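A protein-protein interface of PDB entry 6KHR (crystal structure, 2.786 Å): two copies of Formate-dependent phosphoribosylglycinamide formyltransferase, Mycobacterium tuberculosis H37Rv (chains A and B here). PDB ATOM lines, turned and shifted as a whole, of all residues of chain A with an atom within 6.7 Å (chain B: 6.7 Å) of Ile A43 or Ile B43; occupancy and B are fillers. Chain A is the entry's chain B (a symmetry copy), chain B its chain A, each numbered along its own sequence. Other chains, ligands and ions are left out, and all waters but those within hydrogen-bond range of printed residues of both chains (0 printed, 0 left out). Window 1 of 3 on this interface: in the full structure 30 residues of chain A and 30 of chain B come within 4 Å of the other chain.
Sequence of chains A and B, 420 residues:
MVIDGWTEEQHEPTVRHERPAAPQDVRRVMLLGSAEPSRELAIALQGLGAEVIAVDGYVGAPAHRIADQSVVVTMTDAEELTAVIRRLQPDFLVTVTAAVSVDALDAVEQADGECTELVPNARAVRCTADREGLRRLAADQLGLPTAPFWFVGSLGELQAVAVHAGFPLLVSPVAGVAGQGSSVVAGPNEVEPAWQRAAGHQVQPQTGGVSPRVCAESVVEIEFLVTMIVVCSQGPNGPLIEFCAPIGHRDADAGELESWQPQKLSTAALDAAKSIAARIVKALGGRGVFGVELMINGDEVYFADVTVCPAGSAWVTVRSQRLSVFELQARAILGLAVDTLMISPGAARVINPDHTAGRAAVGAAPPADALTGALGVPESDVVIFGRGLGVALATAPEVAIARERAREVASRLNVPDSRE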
ATOM      1  N   SER A  38      21.547 -18.247   8.283  1.00  0.00           N
ATOM      2  CA  SER A  38      21.518 -17.216   9.325  1.00  0.00           C
ATOM      3  C   SER A  38      21.932 -15.925   8.652  1.00  0.00           C
ATOM      4  O   SER A  38      21.517 -14.904   9.057  1.00  0.00           O
ATOM      5  CB  SER A  38      22.507 -17.632  10.326  1.00  0.00           C
ATOM      6  OG  SER A  38      22.278 -17.024  11.551  1.00  0.00           O
ATOM      7  N   ARG A  39      22.705 -16.013   7.594  1.00  0.00           N
ATOM      8  CA  ARG A  39      23.121 -14.781   6.934  1.00  0.00           C
ATOM      9  C   ARG A  39      22.000 -14.193   6.083  1.00  0.00           C
ATOM     10  O   ARG A  39      21.758 -12.981   6.113  1.00  0.00           O
ATOM     11  CB  ARG A  39      24.369 -15.013   6.079  1.00  0.00           C
ATOM     12  CG  ARG A  39      24.745 -13.801   5.236  1.00  0.00           C
ATOM     13  CD  ARG A  39      25.885 -14.050   4.248  1.00  0.00           C
ATOM     14  NE  ARG A  39      26.082 -12.891   3.372  1.00  0.00           N
ATOM     15  CZ  ARG A  39      25.593 -12.793   2.137  1.00  0.00           C
ATOM     16  NH1 ARG A  39      24.886 -13.796   1.615  1.00  0.00           N
ATOM     17  NH2 ARG A  39      25.813 -11.699   1.419  1.00  0.00           N
ATOM     18  N   GLU A  40      21.305 -15.034   5.330  1.00  0.00           N
ATOM     19  CA  GLU A  40      20.227 -14.546   4.483  1.00  0.00           C
ATOM     20  C   GLU A  40      19.075 -14.006   5.325  1.00  0.00           C
ATOM     21  O   GLU A  40      18.558 -12.910   5.066  1.00  0.00           O
ATOM     22  CB  GLU A  40      19.761 -15.668   3.540  1.00  0.00           C
ATOM     23  CG  GLU A  40      20.886 -16.351   2.779  1.00  0.00           C
ATOM     24  CD  GLU A  40      21.342 -15.559   1.554  1.00  0.00           C
ATOM     25  OE1 GLU A  40      20.516 -14.807   0.995  1.00  0.00           O
ATOM     26  OE2 GLU A  40      22.523 -15.684   1.152  1.00  0.00           O
ATOM     27  N   LEU A  41      18.659 -14.763   6.346  1.00  0.00           N
ATOM     28  CA  LEU A  41      17.686 -14.259   7.303  1.00  0.00           C
ATOM     29  C   LEU A  41      18.097 -12.890   7.835  1.00  0.00           C
ATOM     30  O   LEU A  41      17.247 -12.015   8.038  1.00  0.00           O
ATOM     31  CB  LEU A  41      17.509 -15.262   8.456  1.00  0.00           C
ATOM     32  CG  LEU A  41      16.576 -14.813   9.588  1.00  0.00           C
ATOM     33  CD1 LEU A  41      15.234 -14.416   9.019  1.00  0.00           C
ATOM     34  CD2 LEU A  41      16.401 -15.837  10.747  1.00  0.00           C
ATOM     35  N   ALA A  42      19.395 -12.682   8.037  1.00  0.00           N
ATOM     36  CA  ALA A  42      19.851 -11.431   8.620  1.00  0.00           C
ATOM     37  C   ALA A  42      19.716 -10.286   7.625  1.00  0.00           C
ATOM     38  O   ALA A  42      19.354  -9.158   7.996  1.00  0.00           O
ATOM     39  CB  ALA A  42      21.290 -11.578   9.103  1.00  0.00           C
ATOM     40  N   ILE A  43      20.009 -10.561   6.356  1.00  0.00           N
ATOM     41  CA  ILE A  43      19.757  -9.579   5.313  1.00  0.00           C
ATOM     42  C   ILE A  43      18.275  -9.250   5.282  1.00  0.00           C
ATOM     43  O   ILE A  43      17.878  -8.083   5.341  1.00  0.00           O
ATOM     44  CB  ILE A  43      20.253 -10.105   3.954  1.00  0.00           C
ATOM     45  CG1 ILE A  43      21.778 -10.096   3.894  1.00  0.00           C
ATOM     46  CG2 ILE A  43      19.626  -9.339   2.793  1.00  0.00           C
ATOM     47  CD1 ILE A  43      22.336 -10.946   2.748  1.00  0.00           C
ATOM     48  N   ALA A  44      17.435 -10.287   5.234  1.00  0.00           N
ATOM     49  CA  ALA A  44      15.993 -10.078   5.176  1.00  0.00           C
ATOM     50  C   ALA A  44      15.528  -9.176   6.309  1.00  0.00           C
ATOM     51  O   ALA A  44      14.836  -8.182   6.072  1.00  0.00           O
ATOM     52  CB  ALA A  44      15.258 -11.417   5.208  1.00  0.00           C
ATOM     53  N   LEU A  45      15.944  -9.488   7.545  1.00  0.00           N
ATOM     54  CA  LEU A  45      15.505  -8.713   8.700  1.00  0.00           C
ATOM     55  C   LEU A  45      15.988  -7.272   8.626  1.00  0.00           C
ATOM     56  O   LEU A  45      15.370  -6.380   9.223  1.00  0.00           O
ATOM     57  CB  LEU A  45      16.022  -9.348   9.984  1.00  0.00           C
ATOM     58  CG  LEU A  45      15.302 -10.583  10.480  1.00  0.00           C
ATOM     59  CD1 LEU A  45      16.146 -11.269  11.525  1.00  0.00           C
ATOM     60  CD2 LEU A  45      13.975 -10.162  11.041  1.00  0.00           C
ATOM     61  N   GLN A  46      17.104  -7.031   7.928  1.00  0.00           N
ATOM     62  CA  GLN A  46      17.643  -5.680   7.859  1.00  0.00           C
ATOM     63  C   GLN A  46      16.920  -4.853   6.813  1.00  0.00           C
ATOM     64  O   GLN A  46      16.797  -3.636   6.975  1.00  0.00           O
ATOM     65  CB  GLN A  46      19.145  -5.718   7.588  1.00  0.00           C
ATOM     66  CG  GLN A  46      19.959  -6.051   8.829  1.00  0.00           C
ATOM     67  CD  GLN A  46      21.404  -6.350   8.486  1.00  0.00           C
ATOM     68  OE1 GLN A  46      21.757  -6.430   7.312  1.00  0.00           O
ATOM     69  NE2 GLN A  46      22.245  -6.514   9.503  1.00  0.00           N
ATOM     70  N   GLY A  47      16.408  -5.504   5.766  1.00  0.00           N
ATOM     71  CA  GLY A  47      15.554  -4.806   4.822  1.00  0.00           C
ATOM     72  C   GLY A  47      14.267  -4.311   5.454  1.00  0.00           C
ATOM     73  O   GLY A  47      13.713  -3.289   5.040  1.00  0.00           O
ATOM     74  N   LEU A  48      13.765  -5.026   6.460  1.00  0.00           N
ATOM     75  CA  LEU A  48      12.541  -4.629   7.138  1.00  0.00           C
ATOM     76  C   LEU A  48      12.809  -3.665   8.275  1.00  0.00           C
ATOM     77  O   LEU A  48      11.870  -3.304   8.986  1.00  0.00           O
ATOM     78  CB  LEU A  48      11.797  -5.856   7.671  1.00  0.00           C
ATOM     79  CG  LEU A  48      11.256  -6.928   6.722  1.00  0.00           C
ATOM     80  CD1 LEU A  48      10.795  -8.192   7.496  1.00  0.00           C
ATOM     81  CD2 LEU A  48      10.115  -6.382   5.902  1.00  0.00           C
ATOM     82  N   VAL A  52      20.316  -6.625  13.812  1.00  0.00           N
ATOM     83  CA  VAL A  52      20.479  -8.049  14.096  1.00  0.00           C
ATOM     84  C   VAL A  52      21.800  -8.300  14.810  1.00  0.00           C
ATOM     85  O   VAL A  52      22.854  -7.814  14.384  1.00  0.00           O
ATOM     86  CB  VAL A  52      20.406  -8.919  12.828  1.00  0.00           C
ATOM     87  CG1 VAL A  52      20.687 -10.374  13.206  1.00  0.00           C
ATOM     88  CG2 VAL A  52      19.045  -8.776  12.165  1.00  0.00           C
ATOM     89  N   ILE A  66      27.942  -9.515   8.085  1.00  0.00           N
ATOM     90  CA  ILE A  66      26.991  -8.476   7.709  1.00  0.00           C
ATOM     91  C   ILE A  66      26.049  -8.121   8.834  1.00  0.00           C
ATOM     92  O   ILE A  66      25.215  -7.221   8.664  1.00  0.00           O
ATOM     93  CB  ILE A  66      26.200  -8.870   6.445  1.00  0.00           C
ATOM     94  CG1 ILE A  66      25.146  -9.933   6.763  1.00  0.00           C
ATOM     95  CG2 ILE A  66      27.166  -9.297   5.325  1.00  0.00           C
ATOM     96  CD1 ILE A  66      23.730  -9.381   6.840  1.00  0.00           C
ATOM     97  N   ALA A 330      11.852 -13.875   8.306  1.00  0.00           N
ATOM     98  CA  ALA A 330      12.001 -12.516   8.800  1.00  0.00           C
ATOM     99  C   ALA A 330      10.641 -11.918   9.147  1.00  0.00           C
ATOM    100  O   ALA A 330      10.475 -11.329  10.225  1.00  0.00           O
ATOM    101  CB  ALA A 330      12.740 -11.645   7.784  1.00  0.00           C
ATOM    102  N   SER B  38      24.495   1.200  -3.174  1.00  0.00           N
ATOM    103  CA  SER B  38      25.806   0.613  -2.930  1.00  0.00           C
ATOM    104  C   SER B  38      25.712  -0.581  -1.975  1.00  0.00           C
ATOM    105  O   SER B  38      26.476  -1.545  -2.111  1.00  0.00           O
ATOM    106  CB  SER B  38      26.731   1.698  -2.381  1.00  0.00           C
ATOM    107  OG  SER B  38      28.080   1.286  -2.361  1.00  0.00           O
ATOM    108  N   ARG B  39      24.769  -0.558  -1.025  1.00  0.00           N
ATOM    109  CA  ARG B  39      24.659  -1.678  -0.095  1.00  0.00           C
ATOM    110  C   ARG B  39      24.062  -2.909  -0.767  1.00  0.00           C
ATOM    111  O   ARG B  39      24.554  -4.026  -0.577  1.00  0.00           O
ATOM    112  CB  ARG B  39      23.830  -1.290   1.131  1.00  0.00           C
ATOM    113  CG  ARG B  39      23.542  -2.469   2.049  1.00  0.00           C
ATOM    114  CD  ARG B  39      22.581  -2.154   3.197  1.00  0.00           C
ATOM    115  NE  ARG B  39      22.236  -3.368   3.940  1.00  0.00           N
ATOM    116  CZ  ARG B  39      21.119  -4.070   3.751  1.00  0.00           C
ATOM    117  NH1 ARG B  39      20.219  -3.668   2.854  1.00  0.00           N
ATOM    118  NH2 ARG B  39      20.896  -5.168   4.466  1.00  0.00           N
ATOM    119  N   GLU B  40      23.012  -2.720  -1.557  1.00  0.00           N
ATOM    120  CA  GLU B  40      22.381  -3.851  -2.224  1.00  0.00           C
ATOM    121  C   GLU B  40      23.323  -4.470  -3.255  1.00  0.00           C
ATOM    122  O   GLU B  40      23.489  -5.694  -3.303  1.00  0.00           O
ATOM    123  CB  GLU B  40      21.059  -3.397  -2.866  1.00  0.00           C
ATOM    124  CG  GLU B  40      20.137  -2.642  -1.923  1.00  0.00           C
ATOM    125  CD  GLU B  40      19.338  -3.565  -1.003  1.00  0.00           C
ATOM    126  OE1 GLU B  40      19.084  -4.721  -1.404  1.00  0.00           O
ATOM    127  OE2 GLU B  40      18.964  -3.136   0.115  1.00  0.00           O
ATOM    128  N   LEU B  41      23.949  -3.630  -4.089  1.00  0.00           N
ATOM    129  CA  LEU B  41      24.984  -4.110  -4.989  1.00  0.00           C
ATOM    130  C   LEU B  41      26.024  -4.933  -4.238  1.00  0.00           C
ATOM    131  O   LEU B  41      26.520  -5.942  -4.757  1.00  0.00           O
ATOM    132  CB  LEU B  41      25.649  -2.921  -5.709  1.00  0.00           C
ATOM    133  CG  LEU B  41      26.830  -3.277  -6.621  1.00  0.00           C
ATOM    134  CD1 LEU B  41      26.409  -4.337  -7.618  1.00  0.00           C
ATOM    135  CD2 LEU B  41      27.488  -2.073  -7.352  1.00  0.00           C
ATOM    136  N   ALA B  42      26.344  -4.538  -3.007  1.00  0.00           N
ATOM    137  CA  ALA B  42      27.388  -5.228  -2.265  1.00  0.00           C
ATOM    138  C   ALA B  42      26.912  -6.601  -1.812  1.00  0.00           C
ATOM    139  O   ALA B  42      27.679  -7.576  -1.826  1.00  0.00           O
ATOM    140  CB  ALA B  42      27.830  -4.374  -1.080  1.00  0.00           C
ATOM    141  N   ILE B  43      25.650  -6.693  -1.399  1.00  0.00           N
ATOM    142  CA  ILE B  43      25.064  -7.991  -1.102  1.00  0.00           C
ATOM    143  C   ILE B  43      25.104  -8.858  -2.347  1.00  0.00           C
ATOM    144  O   ILE B  43      25.599  -9.989  -2.320  1.00  0.00           O
ATOM    145  CB  ILE B  43      23.629  -7.815  -0.572  1.00  0.00           C
ATOM    146  CG1 ILE B  43      23.640  -7.249   0.844  1.00  0.00           C
ATOM    147  CG2 ILE B  43      22.836  -9.116  -0.670  1.00  0.00           C
ATOM    148  CD1 ILE B  43      22.273  -6.704   1.277  1.00  0.00           C
ATOM    149  N   ALA B  44      24.623  -8.315  -3.469  1.00  0.00           N
ATOM    150  CA  ALA B  44      24.595  -9.075  -4.713  1.00  0.00           C
ATOM    151  C   ALA B  44      25.972  -9.633  -5.038  1.00  0.00           C
ATOM    152  O   ALA B  44      26.117 -10.832  -5.291  1.00  0.00           O
ATOM    153  CB  ALA B  44      24.075  -8.205  -5.852  1.00  0.00           C
ATOM    154  N   LEU B  45      27.003  -8.779  -4.992  1.00  0.00           N
ATOM    155  CA  LEU B  45      28.351  -9.214  -5.342  1.00  0.00           C
ATOM    156  C   LEU B  45      28.867 -10.281  -4.389  1.00  0.00           C
ATOM    157  O   LEU B  45      29.738 -11.077  -4.762  1.00  0.00           O
ATOM    158  CB  LEU B  45      29.304  -8.024  -5.325  1.00  0.00           C
ATOM    159  CG  LEU B  45      29.248  -7.079  -6.508  1.00  0.00           C
ATOM    160  CD1 LEU B  45      29.976  -5.806  -6.158  1.00  0.00           C
ATOM    161  CD2 LEU B  45      29.875  -7.761  -7.685  1.00  0.00           C
ATOM    162  N   GLN B  46      28.362 -10.294  -3.148  1.00  0.00           N
ATOM    163  CA  GLN B  46      28.845 -11.262  -2.174  1.00  0.00           C
ATOM    164  C   GLN B  46      28.177 -12.608  -2.362  1.00  0.00           C
ATOM    165  O   GLN B  46      28.798 -13.640  -2.088  1.00  0.00           O
ATOM    166  CB  GLN B  46      28.640 -10.737  -0.758  1.00  0.00           C
ATOM    167  CG  GLN B  46      29.682  -9.705  -0.355  1.00  0.00           C
ATOM    168  CD  GLN B  46      29.311  -9.010   0.937  1.00  0.00           C
ATOM    169  OE1 GLN B  46      28.212  -9.210   1.452  1.00  0.00           O
ATOM    170  NE2 GLN B  46      30.216  -8.190   1.468  1.00  0.00           N
ATOM    171  N   GLY B  47      26.939 -12.615  -2.864  1.00  0.00           N
ATOM    172  CA  GLY B  47      26.308 -13.869  -3.235  1.00  0.00           C
ATOM    173  C   GLY B  47      27.035 -14.573  -4.368  1.00  0.00           C
ATOM    174  O   GLY B  47      27.030 -15.805  -4.445  1.00  0.00           O
ATOM    175  N   LEU B  48      27.660 -13.808  -5.261  1.00  0.00           N
ATOM    176  CA  LEU B  48      28.388 -14.394  -6.376  1.00  0.00           C
ATOM    177  C   LEU B  48      29.823 -14.719  -6.007  1.00  0.00           C
ATOM    178  O   LEU B  48      30.582 -15.147  -6.877  1.00  0.00           O
ATOM    179  CB  LEU B  48      28.370 -13.452  -7.584  1.00  0.00           C
ATOM    180  CG  LEU B  48      27.060 -13.073  -8.274  1.00  0.00           C
ATOM    181  CD1 LEU B  48      27.258 -11.907  -9.276  1.00  0.00           C
ATOM    182  CD2 LEU B  48      26.475 -14.267  -8.985  1.00  0.00           C
ATOM    183  N   VAL B  52      34.059  -7.356  -1.147  1.00  0.00           N
ATOM    184  CA  VAL B  52      33.771  -5.981  -1.542  1.00  0.00           C
ATOM    185  C   VAL B  52      34.381  -5.005  -0.544  1.00  0.00           C
ATOM    186  O   VAL B  52      34.222  -5.156   0.673  1.00  0.00           O
ATOM    187  CB  VAL B  52      32.263  -5.703  -1.672  1.00  0.00           C
ATOM    188  CG1 VAL B  52      32.054  -4.222  -1.985  1.00  0.00           C
ATOM    189  CG2 VAL B  52      31.653  -6.584  -2.752  1.00  0.00           C
ATOM    190  N   ILE B  66      27.959  -3.900   5.939  1.00  0.00           N
ATOM    191  CA  ILE B  66      27.983  -5.286   5.491  1.00  0.00           C
ATOM    192  C   ILE B  66      29.122  -5.570   4.541  1.00  0.00           C
ATOM    193  O   ILE B  66      29.284  -6.721   4.113  1.00  0.00           O
ATOM    194  CB  ILE B  66      26.638  -5.697   4.862  1.00  0.00           C
ATOM    195  CG1 ILE B  66      26.475  -5.087   3.467  1.00  0.00           C
ATOM    196  CG2 ILE B  66      25.476  -5.342   5.809  1.00  0.00           C
ATOM    197  CD1 ILE B  66      26.704  -6.084   2.340  1.00  0.00           C
ATOM    198  N   ALA B 330      25.828  -6.361 -10.409  1.00  0.00           N
ATOM    199  CA  ALA B 330      26.819  -7.295  -9.896  1.00  0.00           C
ATOM    200  C   ALA B 330      27.320  -8.215 -11.007  1.00  0.00           C
ATOM    201  O   ALA B 330      28.533  -8.409 -11.158  1.00  0.00           O
ATOM    202  CB  ALA B 330      26.255  -8.100  -8.728  1.00  0.00           C
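Printed residues of chain B within 4 Å of Ile A43: Ile B43 (3.9 Å). Of chain A, only Ile A43 (3.9 Å) comes within 4 Å of Ile B43. Printed residues of chain A within 4 Å of Ile B66: Ile A66 (3.4 Å). Of the printed residues of chain B, Gln A46 touches Arg B39. Printed residues of chain B within 4 Å of Ile A66: Ile B66 (3.4 Å). Printed residues of chain B within 4 Å of Arg A39: Gln B46. Of the printed residues of chain A, Gln B46 touches Arg A39. The nearest printed residue of chain B that does not touch Gln A46 is Ile B66 (4.2 Å).
The guanidinium group (NH1) of Arg A39 is in salt-bridge range of the side-chain carboxylate (OE2) of Glu A40 (3.1 Å). OE2 of Glu B40 is in salt-bridge range of NH1 of Arg B39, 3.1 Å away. The backbone carbonyl oxygen (O) of Ile B66 sits at hydrogen-bond distance from the side-chain amide nitrogen (NE2) of Gln B46 (3.2 Å). NE2 of Gln A46 lies within hydrogen-bond range of O of Ile A66 (3.2 Å).
Ile A43 touches Ile B43 (CD1 to CG2, 3.9 Å). Ile A66 touches Ile B66 (O to CG2, 3.4 Å).
Arg A39 touches Gln B46, and with the chains exchanged Gln A46 touches Arg B39. Ile A43 touches its own counterpart, Ile B43. Ile B66 touches its own counterpart, Ile A66. 14 positions are printed for both chains. Of the 4 pairs that touch across the chains among the printed residues, 4 have their exchanged pair printed and touching as well.
The guanidinium group of Arg A39 sits at hydrogen-bond distance from the side-chain amide oxygen of Gln B46, at 3.5 Å. OE1 of Gln A46 is in hydrogen-bond range of NH2 of Arg B39 (3.2 Å).
Hydrophobic or aromatic side chains of chain B within 4 Å of the printed part of chain A: Ile B43 and Ile B66. Printed residues of chain A that touch a printed residue of chain B: Arg A39, Ile A43, Gln A46 and Ile A66. Hydrophobic or aromatic side chains of chain A that line the printed part of chain B: Ile A43 and Ile A66. Among the printed residues, 4 pairs touch across the chains.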
